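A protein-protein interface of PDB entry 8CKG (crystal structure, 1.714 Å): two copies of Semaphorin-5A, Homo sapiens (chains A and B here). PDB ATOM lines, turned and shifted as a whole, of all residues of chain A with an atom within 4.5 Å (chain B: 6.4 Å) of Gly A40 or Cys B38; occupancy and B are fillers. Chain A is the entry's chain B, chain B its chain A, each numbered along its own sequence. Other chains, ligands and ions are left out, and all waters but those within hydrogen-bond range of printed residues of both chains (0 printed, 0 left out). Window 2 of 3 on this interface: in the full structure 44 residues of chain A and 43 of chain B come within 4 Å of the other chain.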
ATOM      1  N   TRP A   8      -9.673  -4.718 -29.805  1.00  0.00           N
ATOM      2  CA  TRP A   8     -11.055  -4.365 -30.106  1.00  0.00           C
ATOM      3  C   TRP A   8     -11.716  -5.449 -30.943  1.00  0.00           C
ATOM      4  O   TRP A   8     -11.088  -6.052 -31.819  1.00  0.00           O
ATOM      5  CB  TRP A   8     -11.129  -3.045 -30.879  1.00  0.00           C
ATOM      6  CG  TRP A   8     -10.912  -1.813 -30.071  1.00  0.00           C
ATOM      7  CD1 TRP A   8      -9.922  -0.888 -30.243  1.00  0.00           C
ATOM      8  CD2 TRP A   8     -11.706  -1.353 -28.973  1.00  0.00           C
ATOM      9  NE1 TRP A   8     -10.050   0.120 -29.314  1.00  0.00           N
ATOM     10  CE2 TRP A   8     -11.140  -0.140 -28.527  1.00  0.00           C
ATOM     11  CE3 TRP A   8     -12.840  -1.845 -28.323  1.00  0.00           C
ATOM     12  CZ2 TRP A   8     -11.664   0.578 -27.455  1.00  0.00           C
ATOM     13  CZ3 TRP A   8     -13.362  -1.127 -27.263  1.00  0.00           C
ATOM     14  CH2 TRP A   8     -12.773   0.069 -26.838  1.00  0.00           C
ATOM     15  N   CYS A  38      -8.601  -0.670 -24.208  1.00  0.00           N
ATOM     16  CA  CYS A  38      -8.072  -0.664 -25.562  1.00  0.00           C
ATOM     17  C   CYS A  38      -7.907   0.777 -26.027  1.00  0.00           C
ATOM     18  O   CYS A  38      -8.597   1.688 -25.556  1.00  0.00           O
ATOM     19  CB  CYS A  38      -9.001  -1.428 -26.499  1.00  0.00           C
ATOM     20  SG  CYS A  38      -9.203  -3.209 -26.183  1.00  0.00           S
ATOM     21  N   ALA A  39      -6.959   0.987 -26.939  1.00  0.00           N
ATOM     22  CA  ALA A  39      -6.728   2.326 -27.465  1.00  0.00           C
ATOM     23  C   ALA A  39      -7.970   2.822 -28.184  1.00  0.00           C
ATOM     24  O   ALA A  39      -8.593   2.093 -28.960  1.00  0.00           O
ATOM     25  CB  ALA A  39      -5.533   2.338 -28.417  1.00  0.00           C
ATOM     26  N   GLY A  40      -8.341   4.063 -27.910  1.00  0.00           N
ATOM     27  CA  GLY A  40      -9.520   4.616 -28.533  1.00  0.00           C
ATOM     28  C   GLY A  40     -10.803   4.239 -27.813  1.00  0.00           C
ATOM     29  O   GLY A  40     -10.826   3.854 -26.635  1.00  0.00           O
ATOM     30  N   CYS A  41     -11.892   4.323 -28.569  1.00  0.00           N
ATOM     31  CA  CYS A  41     -13.242   4.432 -28.039  1.00  0.00           C
ATOM     32  C   CYS A  41     -14.079   3.211 -28.414  1.00  0.00           C
ATOM     33  O   CYS A  41     -13.950   2.673 -29.519  1.00  0.00           O
ATOM     34  CB  CYS A  41     -13.889   5.722 -28.569  1.00  0.00           C
ATOM     35  SG  CYS A  41     -15.522   6.107 -27.947  1.00  0.00           S
ATOM     36  N   ASN A  42     -14.941   2.774 -27.492  1.00  0.00           N
ATOM     37  CA  ASN A  42     -15.789   1.619 -27.761  1.00  0.00           C
ATOM     38  C   ASN A  42     -17.005   1.954 -28.617  1.00  0.00           C
ATOM     39  O   ASN A  42     -17.742   1.036 -28.993  1.00  0.00           O
ATOM     40  CB  ASN A  42     -16.257   0.972 -26.449  1.00  0.00           C
ATOM     41  CG  ASN A  42     -16.992   1.944 -25.533  1.00  0.00           C
ATOM     42  OD1 ASN A  42     -17.278   3.084 -25.899  1.00  0.00           O
ATOM     43  ND2 ASN A  42     -17.296   1.486 -24.326  1.00  0.00           N
ATOM     44  N   MET B   6       0.885  10.315 -22.903  1.00  0.00           N
ATOM     45  CA  MET B   6      -0.461  10.555 -23.415  1.00  0.00           C
ATOM     46  C   MET B   6      -1.513  10.580 -22.310  1.00  0.00           C
ATOM     47  O   MET B   6      -1.740   9.578 -21.636  1.00  0.00           O
ATOM     48  CB  MET B   6      -0.855   9.488 -24.429  1.00  0.00           C
ATOM     49  CG  MET B   6       0.089   9.315 -25.584  1.00  0.00           C
ATOM     50  SD  MET B   6      -0.675   8.195 -26.762  1.00  0.00           S
ATOM     51  CE  MET B   6       0.720   7.805 -27.810  1.00  0.00           C
ATOM     52  N   PHE B   7      -2.172  11.723 -22.146  1.00  0.00           N
ATOM     53  CA  PHE B   7      -3.235  11.874 -21.164  1.00  0.00           C
ATOM     54  C   PHE B   7      -4.315  12.779 -21.742  1.00  0.00           C
ATOM     55  O   PHE B   7      -4.011  13.736 -22.460  1.00  0.00           O
ATOM     56  CB  PHE B   7      -2.696  12.461 -19.853  1.00  0.00           C
ATOM     57  CG  PHE B   7      -1.913  13.729 -20.042  1.00  0.00           C
ATOM     58  CD1 PHE B   7      -0.549  13.686 -20.301  1.00  0.00           C
ATOM     59  CD2 PHE B   7      -2.540  14.964 -19.982  1.00  0.00           C
ATOM     60  CE1 PHE B   7       0.175  14.850 -20.487  1.00  0.00           C
ATOM     61  CE2 PHE B   7      -1.825  16.132 -20.167  1.00  0.00           C
ATOM     62  CZ  PHE B   7      -0.463  16.075 -20.422  1.00  0.00           C
ATOM     63  N   TRP B   8      -5.572  12.468 -21.435  1.00  0.00           N
ATOM     64  CA  TRP B   8      -6.665  13.333 -21.856  1.00  0.00           C
ATOM     65  C   TRP B   8      -6.613  14.660 -21.113  1.00  0.00           C
ATOM     66  O   TRP B   8      -6.178  14.737 -19.961  1.00  0.00           O
ATOM     67  CB  TRP B   8      -8.024  12.689 -21.586  1.00  0.00           C
ATOM     68  CG  TRP B   8      -8.315  11.419 -22.319  1.00  0.00           C
ATOM     69  CD1 TRP B   8      -8.338  10.159 -21.786  1.00  0.00           C
ATOM     70  CD2 TRP B   8      -8.668  11.279 -23.706  1.00  0.00           C
ATOM     71  NE1 TRP B   8      -8.668   9.241 -22.763  1.00  0.00           N
ATOM     72  CE2 TRP B   8      -8.880   9.902 -23.945  1.00  0.00           C
ATOM     73  CE3 TRP B   8      -8.819  12.181 -24.767  1.00  0.00           C
ATOM     74  CZ2 TRP B   8      -9.224   9.405 -25.208  1.00  0.00           C
ATOM     75  CZ3 TRP B   8      -9.168  11.684 -26.022  1.00  0.00           C
ATOM     76  CH2 TRP B   8      -9.367  10.311 -26.228  1.00  0.00           C
ATOM     77  N   ILE B  31      -9.187  16.381 -25.599  1.00  0.00           N
ATOM     78  CA  ILE B  31      -8.074  16.114 -26.504  1.00  0.00           C
ATOM     79  C   ILE B  31      -7.053  15.225 -25.807  1.00  0.00           C
ATOM     80  O   ILE B  31      -6.758  15.414 -24.623  1.00  0.00           O
ATOM     81  CB  ILE B  31      -7.412  17.420 -26.989  1.00  0.00           C
ATOM     82  N   CYS B  32      -6.524  14.253 -26.543  1.00  0.00           N
ATOM     83  CA  CYS B  32      -5.451  13.401 -26.036  1.00  0.00           C
ATOM     84  C   CYS B  32      -4.117  14.078 -26.323  1.00  0.00           C
ATOM     85  O   CYS B  32      -3.641  14.081 -27.459  1.00  0.00           O
ATOM     86  CB  CYS B  32      -5.508  12.020 -26.676  1.00  0.00           C
ATOM     87  SG  CYS B  32      -4.132  10.940 -26.196  1.00  0.00           S
ATOM     88  N   GLU B  33      -3.503  14.645 -25.290  1.00  0.00           N
ATOM     89  CA  GLU B  33      -2.241  15.349 -25.459  1.00  0.00           C
ATOM     90  C   GLU B  33      -1.077  14.371 -25.555  1.00  0.00           C
ATOM     91  O   GLU B  33      -1.077  13.313 -24.918  1.00  0.00           O
ATOM     92  CB  GLU B  33      -2.014  16.320 -24.301  1.00  0.00           C
ATOM     93  CG  GLU B  33      -2.902  17.557 -24.355  1.00  0.00           C
ATOM     94  CD  GLU B  33      -2.468  18.637 -23.380  1.00  0.00           C
ATOM     95  OE1 GLU B  33      -1.843  18.294 -22.357  1.00  0.00           O
ATOM     96  OE2 GLU B  33      -2.743  19.830 -23.640  1.00  0.00           O
ATOM     97  N   GLY B  35       0.033  12.517 -28.070  1.00  0.00           N
ATOM     98  CA  GLY B  35      -0.158  11.283 -28.794  1.00  0.00           C
ATOM     99  C   GLY B  35      -1.608  11.063 -29.159  1.00  0.00           C
ATOM    100  O   GLY B  35      -2.501  11.775 -28.691  1.00  0.00           O
ATOM    101  N   PRO B  36      -1.875  10.070 -30.007  1.00  0.00           N
ATOM    102  CA  PRO B  36      -3.260   9.822 -30.428  1.00  0.00           C
ATOM    103  C   PRO B  36      -4.015   8.852 -29.528  1.00  0.00           C
ATOM    104  O   PRO B  36      -5.235   8.971 -29.371  1.00  0.00           O
ATOM    105  CB  PRO B  36      -3.088   9.238 -31.834  1.00  0.00           C
ATOM    106  CG  PRO B  36      -1.784   8.496 -31.750  1.00  0.00           C
ATOM    107  CD  PRO B  36      -0.911   9.260 -30.772  1.00  0.00           C
ATOM    108  N   ASP B  37      -3.302   7.910 -28.920  1.00  0.00           N
ATOM    109  CA  ASP B  37      -3.904   6.681 -28.393  1.00  0.00           C
ATOM    110  C   ASP B  37      -4.136   6.722 -26.886  1.00  0.00           C
ATOM    111  O   ASP B  37      -3.752   5.795 -26.171  1.00  0.00           O
ATOM    112  CB  ASP B  37      -3.035   5.484 -28.763  1.00  0.00           C
ATOM    113  CG  ASP B  37      -3.089   5.158 -30.238  1.00  0.00           C
ATOM    114  OD1 ASP B  37      -3.961   5.707 -30.948  1.00  0.00           O
ATOM    115  OD2 ASP B  37      -2.252   4.345 -30.683  1.00  0.00           O
ATOM    116  N   CYS B  38      -4.777   7.766 -26.367  1.00  0.00           N
ATOM    117  CA  CYS B  38      -5.287   7.678 -25.006  1.00  0.00           C
ATOM    118  C   CYS B  38      -6.407   6.644 -24.959  1.00  0.00           C
ATOM    119  O   CYS B  38      -7.090   6.396 -25.954  1.00  0.00           O
ATOM    120  CB  CYS B  38      -5.806   9.029 -24.520  1.00  0.00           C
ATOM    121  SG  CYS B  38      -4.592  10.340 -24.299  1.00  0.00           S
ATOM    122  N   ALA B  39      -6.590   6.030 -23.796  1.00  0.00           N
ATOM    123  CA  ALA B  39      -7.653   5.048 -23.637  1.00  0.00           C
ATOM    124  C   ALA B  39      -8.987   5.744 -23.400  1.00  0.00           C
ATOM    125  O   ALA B  39      -9.123   6.559 -22.482  1.00  0.00           O
ATOM    126  CB  ALA B  39      -7.338   4.103 -22.484  1.00  0.00           C
ATOM    127  N   GLY B  40      -9.970   5.415 -24.218  1.00  0.00           N
ATOM    128  CA  GLY B  40     -11.294   5.969 -24.069  1.00  0.00           C
ATOM    129  C   GLY B  40     -11.683   6.862 -25.228  1.00  0.00           C
ATOM    130  O   GLY B  40     -11.115   6.801 -26.322  1.00  0.00           O
ATOM    131  N   CYS B  41     -12.650   7.737 -24.963  1.00  0.00           N
ATOM    132  CA  CYS B  41     -13.337   8.493 -25.994  1.00  0.00           C
ATOM    133  C   CYS B  41     -13.051   9.980 -25.848  1.00  0.00           C
ATOM    134  O   CYS B  41     -12.847  10.491 -24.739  1.00  0.00           O
ATOM    135  CB  CYS B  41     -14.846   8.240 -25.921  1.00  0.00           C
ATOM    136  SG  CYS B  41     -15.268   6.489 -25.967  1.00  0.00           S
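N of Cys A41 is in hydrogen-bond range of O of Gly B40 (3.4 Å).
The backbone NH of Gly B40 is in hydrogen-bond range of the backbone carbonyl oxygen of Gly A40 (3.0 Å).
The backbone carbonyl oxygen (O) of Cys B38 lies within hydrogen-bond range of the backbone NH (N) of Gly A40, at 3.3 Å.
The side-chain sulfur of Cys B41 forms a disulfide with the side-chain sulfur of Cys A41, at 2.0 Å.
The backbone NH (N) of Phe B7 lies within hydrogen-bond range of the side-chain sulfur (SG) of Cys B38.
The side-chain sulfur (SG) of Cys B38 forms a disulfide with the side-chain sulfur (SG) of Cys B32, 2.0 Å away.
The backbone NH (N) of Trp B8 sits at hydrogen-bond distance from the side-chain sulfur (SG) of Cys B38 (3.7 Å).
The indole nitrogen (NE1) of Trp B8 is in hydrogen-bond range of the backbone carbonyl oxygen (O) of Ala B39 (2.7 Å).
Ala B39 touches Cys A38.
Cys B41 touches Asn A42 (SG to OD1, 3.95 Å).
Of chain B, only Cys B38 (3.3 Å) and Gly B40 (3.0 Å) come within 4 Å of Gly A40.
Of the printed residues of chain A, Cys B38 touches Gly A40.
Printed residues of chain A within 4 Å of Ala B39: Cys A38.
Printed residues of chain B within 4 Å of Asn A42: Cys B41.
Printed residues of chain A within 4 Å of Cys B41: Cys A41 and Asn A42.
Trp A8 touches none of the printed residues of chain B.
Of the 6 printed residues of chain A, 4 touch a printed residue of chain B.
Printed residues of chain A that touch a printed residue of chain B: Cys A38, Gly A40, Cys A41 and Asn A42.
Of the 13 printed residues of chain B, 4 touch a printed residue of chain A.
Among the printed residues, no Asp or Glu carboxylate lies within 4 Å of a Lys or Arg side-chain nitrogen of the other chain.
Cys A38 touches Ala B39, but with the chains exchanged Ala A39 does not touch Cys B38 (4.3 Å).
Gly A40 touches Cys B38, but with the chains exchanged Cys A38 does not touch Gly B40 (4.2 Å).
Gly A40 touches its own counterpart, Gly B40.
Cys A41 touches its own counterpart, Cys B41.
5 positions are printed for both chains.
Of the 6 pairs that touch across the chains among the printed residues, 2 have their exchanged pair printed and touching as well.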
